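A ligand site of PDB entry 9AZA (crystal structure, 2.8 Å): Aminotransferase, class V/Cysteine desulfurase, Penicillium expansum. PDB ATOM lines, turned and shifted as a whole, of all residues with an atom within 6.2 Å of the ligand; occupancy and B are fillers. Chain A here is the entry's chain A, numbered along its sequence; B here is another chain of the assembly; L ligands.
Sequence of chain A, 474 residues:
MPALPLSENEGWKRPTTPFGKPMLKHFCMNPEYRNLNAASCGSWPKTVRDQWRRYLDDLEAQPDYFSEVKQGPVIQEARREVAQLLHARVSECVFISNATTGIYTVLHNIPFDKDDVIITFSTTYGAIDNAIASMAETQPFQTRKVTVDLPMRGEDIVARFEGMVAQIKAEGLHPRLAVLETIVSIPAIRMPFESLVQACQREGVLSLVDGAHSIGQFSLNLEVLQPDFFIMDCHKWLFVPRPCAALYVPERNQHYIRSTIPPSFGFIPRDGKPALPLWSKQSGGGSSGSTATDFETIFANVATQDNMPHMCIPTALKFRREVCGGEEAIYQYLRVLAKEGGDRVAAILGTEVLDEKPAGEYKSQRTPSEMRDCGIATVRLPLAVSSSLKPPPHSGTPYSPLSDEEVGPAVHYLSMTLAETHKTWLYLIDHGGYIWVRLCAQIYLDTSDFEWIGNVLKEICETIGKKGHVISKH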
ATOM      1  N   ALA A  39     -36.738 -17.873 -21.900  1.00  0.00           N
ATOM      2  CA  ALA A  39     -35.774 -18.479 -22.827  1.00  0.00           C
ATOM      3  C   ALA A  39     -34.567 -19.060 -22.109  1.00  0.00           C
ATOM      4  O   ALA A  39     -33.417 -18.824 -22.497  1.00  0.00           O
ATOM      5  CB  ALA A  39     -35.356 -17.448 -23.869  1.00  0.00           C
ATOM      6  N   SER A  97     -29.140 -32.987 -28.488  1.00  0.00           N
ATOM      7  CA  SER A  97     -29.563 -32.722 -27.116  1.00  0.00           C
ATOM      8  C   SER A  97     -29.617 -31.228 -26.792  1.00  0.00           C
ATOM      9  O   SER A  97     -30.583 -30.769 -26.187  1.00  0.00           O
ATOM     10  CB  SER A  97     -28.647 -33.449 -26.139  1.00  0.00           C
ATOM     11  OG  SER A  97     -27.526 -32.642 -25.822  1.00  0.00           O
ATOM     12  N   ASN A  98     -28.591 -30.465 -27.182  1.00  0.00           N
ATOM     13  CA  ASN A  98     -28.577 -29.030 -26.889  1.00  0.00           C
ATOM     14  C   ASN A  98     -27.685 -28.323 -27.902  1.00  0.00           C
ATOM     15  O   ASN A  98     -26.973 -28.957 -28.685  1.00  0.00           O
ATOM     16  CB  ASN A  98     -28.109 -28.740 -25.462  1.00  0.00           C
ATOM     17  CG  ASN A  98     -26.880 -29.542 -25.071  1.00  0.00           C
ATOM     18  OD1 ASN A  98     -25.811 -29.395 -25.651  1.00  0.00           O
ATOM     19  ND2 ASN A  98     -27.045 -30.399 -24.073  1.00  0.00           N
ATOM     20  N   ALA A  99     -27.724 -26.980 -27.863  1.00  0.00           N
ATOM     21  CA  ALA A  99     -27.005 -26.191 -28.857  1.00  0.00           C
ATOM     22  C   ALA A  99     -25.493 -26.393 -28.750  1.00  0.00           C
ATOM     23  O   ALA A  99     -24.795 -26.410 -29.764  1.00  0.00           O
ATOM     24  CB  ALA A  99     -27.348 -24.709 -28.716  1.00  0.00           C
ATOM     25  N   THR A 100     -24.977 -26.557 -27.527  1.00  0.00           N
ATOM     26  CA  THR A 100     -23.547 -26.762 -27.358  1.00  0.00           C
ATOM     27  C   THR A 100     -23.076 -28.025 -28.063  1.00  0.00           C
ATOM     28  O   THR A 100     -22.032 -28.029 -28.722  1.00  0.00           O
ATOM     29  CB  THR A 100     -23.204 -26.810 -25.869  1.00  0.00           C
ATOM     30  OG1 THR A 100     -23.545 -25.555 -25.265  1.00  0.00           O
ATOM     31  CG2 THR A 100     -21.718 -27.079 -25.682  1.00  0.00           C
ATOM     32  N   THR A 101     -23.848 -29.123 -27.940  1.00  0.00           N
ATOM     33  CA  THR A 101     -23.435 -30.372 -28.577  1.00  0.00           C
ATOM     34  C   THR A 101     -23.467 -30.266 -30.098  1.00  0.00           C
ATOM     35  O   THR A 101     -22.622 -30.851 -30.774  1.00  0.00           O
ATOM     36  CB  THR A 101     -24.331 -31.524 -28.101  1.00  0.00           C
ATOM     37  OG1 THR A 101     -24.168 -31.700 -26.691  1.00  0.00           O
ATOM     38  CG2 THR A 101     -23.976 -32.832 -28.802  1.00  0.00           C
ATOM     39  N   ILE A 103     -23.153 -27.399 -32.124  1.00  0.00           N
ATOM     40  CA  ILE A 103     -22.043 -26.567 -32.610  1.00  0.00           C
ATOM     41  C   ILE A 103     -20.732 -27.316 -32.494  1.00  0.00           C
ATOM     42  O   ILE A 103     -19.868 -27.254 -33.372  1.00  0.00           O
ATOM     43  CB  ILE A 103     -21.988 -25.239 -31.851  1.00  0.00           C
ATOM     44  CG1 ILE A 103     -23.324 -24.511 -31.928  1.00  0.00           C
ATOM     45  CG2 ILE A 103     -20.861 -24.370 -32.390  1.00  0.00           C
ATOM     46  CD1 ILE A 103     -23.338 -23.198 -31.201  1.00  0.00           C
ATOM     47  N   THR A 123     -18.753 -11.276 -29.216  1.00  0.00           N
ATOM     48  CA  THR A 123     -20.102 -11.689 -28.882  1.00  0.00           C
ATOM     49  C   THR A 123     -20.306 -13.198 -28.902  1.00  0.00           C
ATOM     50  O   THR A 123     -21.374 -13.670 -28.489  1.00  0.00           O
ATOM     51  CB  THR A 123     -21.091 -11.079 -29.867  1.00  0.00           C
ATOM     52  OG1 THR A 123     -20.809 -11.550 -31.192  1.00  0.00           O
ATOM     53  CG2 THR A 123     -20.973  -9.584 -29.847  1.00  0.00           C
ATOM     54  N   TYR A 125     -20.700 -16.888 -28.007  1.00  0.00           N
ATOM     55  CA  TYR A 125     -21.019 -17.560 -26.763  1.00  0.00           C
ATOM     56  C   TYR A 125     -19.772 -18.168 -26.132  1.00  0.00           C
ATOM     57  O   TYR A 125     -18.904 -18.688 -26.819  1.00  0.00           O
ATOM     58  CB  TYR A 125     -22.070 -18.637 -27.015  1.00  0.00           C
ATOM     59  CG  TYR A 125     -22.726 -19.157 -25.764  1.00  0.00           C
ATOM     60  CD1 TYR A 125     -23.565 -18.343 -25.017  1.00  0.00           C
ATOM     61  CD2 TYR A 125     -22.510 -20.450 -25.331  1.00  0.00           C
ATOM     62  CE1 TYR A 125     -24.170 -18.813 -23.866  1.00  0.00           C
ATOM     63  CE2 TYR A 125     -23.116 -20.930 -24.183  1.00  0.00           C
ATOM     64  CZ  TYR A 125     -23.945 -20.108 -23.461  1.00  0.00           C
ATOM     65  OH  TYR A 125     -24.532 -20.586 -22.322  1.00  0.00           O
ATOM     66  N   ILE A 128     -18.579 -21.677 -26.811  1.00  0.00           N
ATOM     67  CA  ILE A 128     -18.016 -21.917 -28.136  1.00  0.00           C
ATOM     68  C   ILE A 128     -16.527 -21.591 -28.148  1.00  0.00           C
ATOM     69  O   ILE A 128     -15.736 -22.271 -28.811  1.00  0.00           O
ATOM     70  CB  ILE A 128     -18.765 -21.093 -29.190  1.00  0.00           C
ATOM     71  CG1 ILE A 128     -20.276 -21.303 -29.042  1.00  0.00           C
ATOM     72  CG2 ILE A 128     -18.313 -21.489 -30.591  1.00  0.00           C
ATOM     73  CD1 ILE A 128     -21.093 -20.460 -29.976  1.00  0.00           C
ATOM     74  N   GLU A 181     -23.889 -15.779 -34.815  1.00  0.00           N
ATOM     75  CA  GLU A 181     -25.021 -16.026 -33.950  1.00  0.00           C
ATOM     76  C   GLU A 181     -26.197 -15.209 -34.466  1.00  0.00           C
ATOM     77  O   GLU A 181     -26.018 -14.162 -35.084  1.00  0.00           O
ATOM     78  CB  GLU A 181     -24.720 -15.638 -32.489  1.00  0.00           C
ATOM     79  CG  GLU A 181     -23.341 -16.044 -32.022  1.00  0.00           C
ATOM     80  CD  GLU A 181     -22.306 -14.946 -32.244  1.00  0.00           C
ATOM     81  OE1 GLU A 181     -22.707 -13.758 -32.348  1.00  0.00           O
ATOM     82  OE2 GLU A 181     -21.099 -15.273 -32.320  1.00  0.00           O
ATOM     83  N   ILE A 183     -29.062 -14.444 -32.146  1.00  0.00           N
ATOM     84  CA  ILE A 183     -29.196 -13.641 -30.933  1.00  0.00           C
ATOM     85  C   ILE A 183     -27.951 -13.869 -30.078  1.00  0.00           C
ATOM     86  O   ILE A 183     -27.691 -15.007 -29.644  1.00  0.00           O
ATOM     87  CB  ILE A 183     -30.463 -14.002 -30.139  1.00  0.00           C
ATOM     88  CG1 ILE A 183     -31.718 -13.515 -30.880  1.00  0.00           C
ATOM     89  CG2 ILE A 183     -30.415 -13.439 -28.727  1.00  0.00           C
ATOM     90  CD1 ILE A 183     -31.523 -12.190 -31.543  1.00  0.00           C
ATOM     91  N   VAL A 184     -27.188 -12.801 -29.857  1.00  0.00           N
ATOM     92  CA  VAL A 184     -26.136 -12.844 -28.842  1.00  0.00           C
ATOM     93  C   VAL A 184     -26.784 -13.154 -27.495  1.00  0.00           C
ATOM     94  O   VAL A 184     -27.842 -12.619 -27.156  1.00  0.00           O
ATOM     95  CB  VAL A 184     -25.364 -11.523 -28.811  1.00  0.00           C
ATOM     96  CG1 VAL A 184     -26.317 -10.361 -28.827  1.00  0.00           C
ATOM     97  CG2 VAL A 184     -24.446 -11.455 -27.587  1.00  0.00           C
ATOM     98  N   SER A 185     -26.148 -14.043 -26.726  1.00  0.00           N
ATOM     99  CA  SER A 185     -26.727 -14.508 -25.468  1.00  0.00           C
ATOM    100  C   SER A 185     -27.062 -13.339 -24.548  1.00  0.00           C
ATOM    101  O   SER A 185     -28.232 -13.101 -24.208  1.00  0.00           O
ATOM    102  CB  SER A 185     -25.764 -15.479 -24.791  1.00  0.00           C
ATOM    103  OG  SER A 185     -24.437 -14.997 -24.821  1.00  0.00           O
ATOM    104  N   ILE A 186     -26.046 -12.581 -24.153  1.00  0.00           N
ATOM    105  CA  ILE A 186     -26.199 -11.406 -23.294  1.00  0.00           C
ATOM    106  C   ILE A 186     -24.923 -10.592 -23.387  1.00  0.00           C
ATOM    107  O   ILE A 186     -23.832 -11.171 -23.220  1.00  0.00           O
ATOM    108  CB  ILE A 186     -26.531 -11.828 -21.846  1.00  0.00           C
ATOM    109  CG1 ILE A 186     -26.399 -10.646 -20.886  1.00  0.00           C
ATOM    110  CG2 ILE A 186     -25.630 -12.979 -21.405  1.00  0.00           C
ATOM    111  CD1 ILE A 186     -27.542  -9.673 -20.987  1.00  0.00           C
ATOM    112  N   ASP A 210     -24.870 -20.054 -34.875  1.00  0.00           N
ATOM    113  CA  ASP A 210     -25.409 -20.355 -33.552  1.00  0.00           C
ATOM    114  C   ASP A 210     -26.743 -19.617 -33.404  1.00  0.00           C
ATOM    115  O   ASP A 210     -26.828 -18.495 -32.912  1.00  0.00           O
ATOM    116  CB  ASP A 210     -24.422 -19.950 -32.469  1.00  0.00           C
ATOM    117  CG  ASP A 210     -25.056 -19.893 -31.085  1.00  0.00           C
ATOM    118  OD1 ASP A 210     -25.975 -20.692 -30.805  1.00  0.00           O
ATOM    119  OD2 ASP A 210     -24.617 -19.036 -30.274  1.00  0.00           O
ATOM    120  N   ALA A 212     -29.222 -20.401 -31.387  1.00  0.00           N
ATOM    121  CA  ALA A 212     -29.857 -20.956 -30.195  1.00  0.00           C
ATOM    122  C   ALA A 212     -31.169 -20.250 -29.929  1.00  0.00           C
ATOM    123  O   ALA A 212     -32.196 -20.893 -29.646  1.00  0.00           O
ATOM    124  CB  ALA A 212     -28.917 -20.852 -28.991  1.00  0.00           C
ATOM    125  N   HIS A 213     -31.168 -18.929 -30.023  1.00  0.00           N
ATOM    126  CA  HIS A 213     -32.402 -18.157 -30.039  1.00  0.00           C
ATOM    127  C   HIS A 213     -32.773 -17.909 -31.487  1.00  0.00           C
ATOM    128  O   HIS A 213     -32.174 -17.060 -32.155  1.00  0.00           O
ATOM    129  CB  HIS A 213     -32.246 -16.848 -29.276  1.00  0.00           C
ATOM    130  CG  HIS A 213     -31.836 -17.016 -27.852  1.00  0.00           C
ATOM    131  ND1 HIS A 213     -32.754 -17.193 -26.840  1.00  0.00           N
ATOM    132  CD2 HIS A 213     -30.619 -16.994 -27.266  1.00  0.00           C
ATOM    133  CE1 HIS A 213     -32.117 -17.281 -25.681  1.00  0.00           C
ATOM    134  NE2 HIS A 213     -30.824 -17.173 -25.915  1.00  0.00           N
ATOM    135  N   ASP A 233     -32.090 -23.952 -30.552  1.00  0.00           N
ATOM    136  CA  ASP A 233     -32.707 -24.494 -29.340  1.00  0.00           C
ATOM    137  C   ASP A 233     -34.213 -24.338 -29.467  1.00  0.00           C
ATOM    138  O   ASP A 233     -34.740 -23.219 -29.397  1.00  0.00           O
ATOM    139  CB  ASP A 233     -32.189 -23.774 -28.105  1.00  0.00           C
ATOM    140  CG  ASP A 233     -31.057 -24.504 -27.430  1.00  0.00           C
ATOM    141  OD1 ASP A 233     -30.747 -25.648 -27.815  1.00  0.00           O
ATOM    142  OD2 ASP A 233     -30.473 -23.915 -26.484  1.00  0.00           O
ATOM    143  N   HIS A 235     -36.414 -25.543 -27.237  1.00  0.00           N
ATOM    144  CA  HIS A 235     -36.992 -25.320 -25.922  1.00  0.00           C
ATOM    145  C   HIS A 235     -36.961 -23.867 -25.467  1.00  0.00           C
ATOM    146  O   HIS A 235     -37.695 -23.498 -24.551  1.00  0.00           O
ATOM    147  CB  HIS A 235     -36.297 -26.201 -24.875  1.00  0.00           C
ATOM    148  CG  HIS A 235     -34.887 -25.777 -24.557  1.00  0.00           C
ATOM    149  ND1 HIS A 235     -33.793 -26.494 -24.992  1.00  0.00           N
ATOM    150  CD2 HIS A 235     -34.400 -24.747 -23.834  1.00  0.00           C
ATOM    151  CE1 HIS A 235     -32.693 -25.904 -24.559  1.00  0.00           C
ATOM    152  NE2 HIS A 235     -33.030 -24.843 -23.853  1.00  0.00           N
ATOM    153  N   LYS A 236     -36.124 -23.050 -26.098  1.00  0.00           N
ATOM    154  CA  LYS A 236     -35.974 -21.666 -25.655  1.00  0.00           C
ATOM    155  C   LYS A 236     -37.175 -20.807 -26.098  1.00  0.00           C
ATOM    156  O   LYS A 236     -37.465 -19.788 -25.465  1.00  0.00           O
ATOM    157  CB  LYS A 236     -34.635 -21.081 -26.155  1.00  0.00           C
ATOM    158  CG  LYS A 236     -33.344 -21.525 -25.426  1.00  0.00           C
ATOM    159  CD  LYS A 236     -32.088 -20.642 -25.530  1.00  0.00           C
ATOM    160  CE  LYS A 236     -30.905 -20.889 -24.572  1.00  0.00           C
ATOM    161  NZ  LYS A 236     -29.653 -20.633 -25.269  1.00  0.00           N
ATOM    162  N   PRO A 243     -34.102 -30.346 -22.295  1.00  0.00           N
ATOM    163  CA  PRO A 243     -33.308 -29.809 -23.406  1.00  0.00           C
ATOM    164  C   PRO A 243     -33.840 -30.251 -24.777  1.00  0.00           C
ATOM    165  O   PRO A 243     -34.181 -31.412 -24.953  1.00  0.00           O
ATOM    166  CB  PRO A 243     -31.917 -30.372 -23.107  1.00  0.00           C
ATOM    167  CG  PRO A 243     -32.205 -31.744 -22.534  1.00  0.00           C
ATOM    168  CD  PRO A 243     -33.531 -31.614 -21.799  1.00  0.00           C
ATOM    169  N   ALA A 245     -33.032 -29.361 -29.055  1.00  0.00           N
ATOM    170  CA  ALA A 245     -32.338 -28.610 -30.087  1.00  0.00           C
ATOM    171  C   ALA A 245     -32.337 -29.417 -31.379  1.00  0.00           C
ATOM    172  O   ALA A 245     -32.557 -30.640 -31.367  1.00  0.00           O
ATOM    173  CB  ALA A 245     -30.897 -28.286 -29.669  1.00  0.00           C
ATOM    174  N   ARG A 438     -31.539  -8.586 -19.038  1.00  0.00           N
ATOM    175  CA  ARG A 438     -32.201  -9.196 -20.188  1.00  0.00           C
ATOM    176  C   ARG A 438     -33.681  -9.422 -19.873  1.00  0.00           C
ATOM    177  O   ARG A 438     -34.013 -10.150 -18.936  1.00  0.00           O
ATOM    178  CB  ARG A 438     -31.538 -10.509 -20.569  1.00  0.00           C
ATOM    179  CG  ARG A 438     -31.844 -10.946 -21.976  1.00  0.00           C
ATOM    180  CD  ARG A 438     -31.224 -12.276 -22.262  1.00  0.00           C
ATOM    181  NE  ARG A 438     -31.811 -13.332 -21.453  1.00  0.00           N
ATOM    182  CZ  ARG A 438     -31.625 -14.627 -21.672  1.00  0.00           C
ATOM    183  NH1 ARG A 438     -30.855 -15.049 -22.661  1.00  0.00           N
ATOM    184  NH2 ARG A 438     -32.211 -15.517 -20.884  1.00  0.00           N
ATOM    185  N   VAL B 302     -22.234 -26.992 -16.941  1.00  0.00           N
ATOM    186  CA  VAL B 302     -22.349 -27.676 -18.227  1.00  0.00           C
ATOM    187  C   VAL B 302     -23.504 -27.081 -18.999  1.00  0.00           C
ATOM    188  O   VAL B 302     -24.201 -26.182 -18.509  1.00  0.00           O
ATOM    189  CB  VAL B 302     -22.513 -29.195 -18.036  1.00  0.00           C
ATOM    190  CG1 VAL B 302     -21.513 -29.732 -17.016  1.00  0.00           C
ATOM    191  CG2 VAL B 302     -23.946 -29.538 -17.635  1.00  0.00           C
ATOM    192  N   ALA B 303     -23.718 -27.553 -20.229  1.00  0.00           N
ATOM    193  CA  ALA B 303     -24.814 -27.061 -21.055  1.00  0.00           C
ATOM    194  C   ALA B 303     -26.158 -27.474 -20.466  1.00  0.00           C
ATOM    195  O   ALA B 303     -26.238 -28.122 -19.420  1.00  0.00           O
ATOM    196  CB  ALA B 303     -24.667 -27.559 -22.489  1.00  0.00           C
ATOM    197  N   THR B 304     -27.227 -27.105 -21.153  1.00  0.00           N
ATOM    198  CA  THR B 304     -28.559 -27.389 -20.638  1.00  0.00           C
ATOM    199  C   THR B 304     -28.847 -28.886 -20.673  1.00  0.00           C
ATOM    200  O   THR B 304     -28.724 -29.532 -21.718  1.00  0.00           O
ATOM    201  CB  THR B 304     -29.619 -26.633 -21.443  1.00  0.00           C
ATOM    202  OG1 THR B 304     -29.078 -25.365 -21.859  1.00  0.00           O
ATOM    203  CG2 THR B 304     -30.843 -26.393 -20.587  1.00  0.00           C
HETATM  204  N1  LIG L   1     -25.278 -19.708 -27.420  1.00  0.00           N
HETATM  205  C1  LIG L   1     -26.172 -18.785 -27.144  1.00  0.00           C
HETATM  206  C2  LIG L   1     -26.047 -17.449 -27.793  1.00  0.00           C
HETATM  207  C3  LIG L   1     -27.237 -19.036 -26.253  1.00  0.00           C
HETATM  208  O1  LIG L   1     -28.102 -18.057 -26.028  1.00  0.00           O
HETATM  209  C4  LIG L   1     -27.354 -20.292 -25.625  1.00  0.00           C
HETATM  210  C5  LIG L   1     -28.488 -20.553 -24.718  1.00  0.00           C
HETATM  211  C6  LIG L   1     -26.383 -21.256 -25.954  1.00  0.00           C
HETATM  212  C7  LIG L   1     -25.388 -20.896 -26.840  1.00  0.00           C
HETATM  213  C8  LIG L   1     -26.313 -22.652 -25.396  1.00  0.00           C
HETATM  214  O2  LIG L   1     -27.515 -23.346 -25.364  1.00  0.00           O
HETATM  215  P1  LIG L   1     -27.429 -24.863 -24.544  1.00  0.00           P
HETATM  216  O3  LIG L   1     -28.823 -25.479 -24.730  1.00  0.00           O
HETATM  217  O4  LIG L   1     -26.331 -25.641 -25.272  1.00  0.00           O
HETATM  218  O5  LIG L   1     -27.087 -24.420 -23.129  1.00  0.00           O
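The side-chain carboxylate of Asp 210 sits close to a nitrogen (N1) of the ligand (3.0 Å). Asn 98 touches the ligand (CB to O3, 3.4 Å). CG of Tyr 125 touches N1 of the ligand, 3.1 Å away. Ile 183 touches the ligand (O to C2, 3.5 Å). Ser 185 touches the ligand. Ala 212 touches the ligand (CB to C3, 3.7 Å). His 235 touches the ligand (CE1 to O3, 3.9 Å). Ala 303 of chain B touches the ligand. Hydrophobic or aromatic side chains within 4 Å of the ligand: Ala 99, Tyr 125, Ala 212, His 213, His 235 and Ala 303 of chain B. Of the 27 residues printed, 14 come within 4 Å of the ligand.
A carbon (C5) of the ligand is bonded to the side-chain amino group of Lys 236 (1.3 Å). The backbone NH of Thr 304 of chain B is in hydrogen-bond range of an oxygen (O5) of the ligand (3.3 Å). The side-chain hydroxyl of Thr 304 of chain B sits at hydrogen-bond distance from an oxygen (O5) of the ligand (2.5 Å). An oxygen (O4) of the ligand sits at hydrogen-bond distance from the backbone NH of Thr 100 (2.8 Å). The side-chain hydroxyl (OG1) of Thr 100 is in hydrogen-bond range of an oxygen (O4) of the ligand, 2.8 Å away. A ring nitrogen (NE2) of His 213 is in hydrogen-bond range of an oxygen (O1) of the ligand (2.9 Å). An oxygen (O3) of the ligand sits close to the side-chain carboxylate of Asp 233, at 2.9 Å. The backbone NH (N) of Ala 99 sits at hydrogen-bond distance from an oxygen (O4) of the ligand.
The side-chain carboxylate (OD2) of Asp 233 lies within salt-bridge range of the side-chain amino group (NZ) of Lys 236 (3.6 Å). ND2 of Asn 98 sits at hydrogen-bond distance from O of Thr 304 of chain B (3.0 Å). OD1 of Asp 233 sits at hydrogen-bond distance from N of Ala 99. O of Ala 212 is in hydrogen-bond range of N of Asp 233, at 3.2 Å. The backbone NH of Ala 212 lies close to the side-chain carboxylate of Asp 210 (3.3 Å). The side-chain amide oxygen of Asn 98 sits at hydrogen-bond distance from the side-chain hydroxyl of Thr 101 (3.0 Å). OG of Ser 97 is in hydrogen-bond range of ND2 of Asn 98 (2.9 Å).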
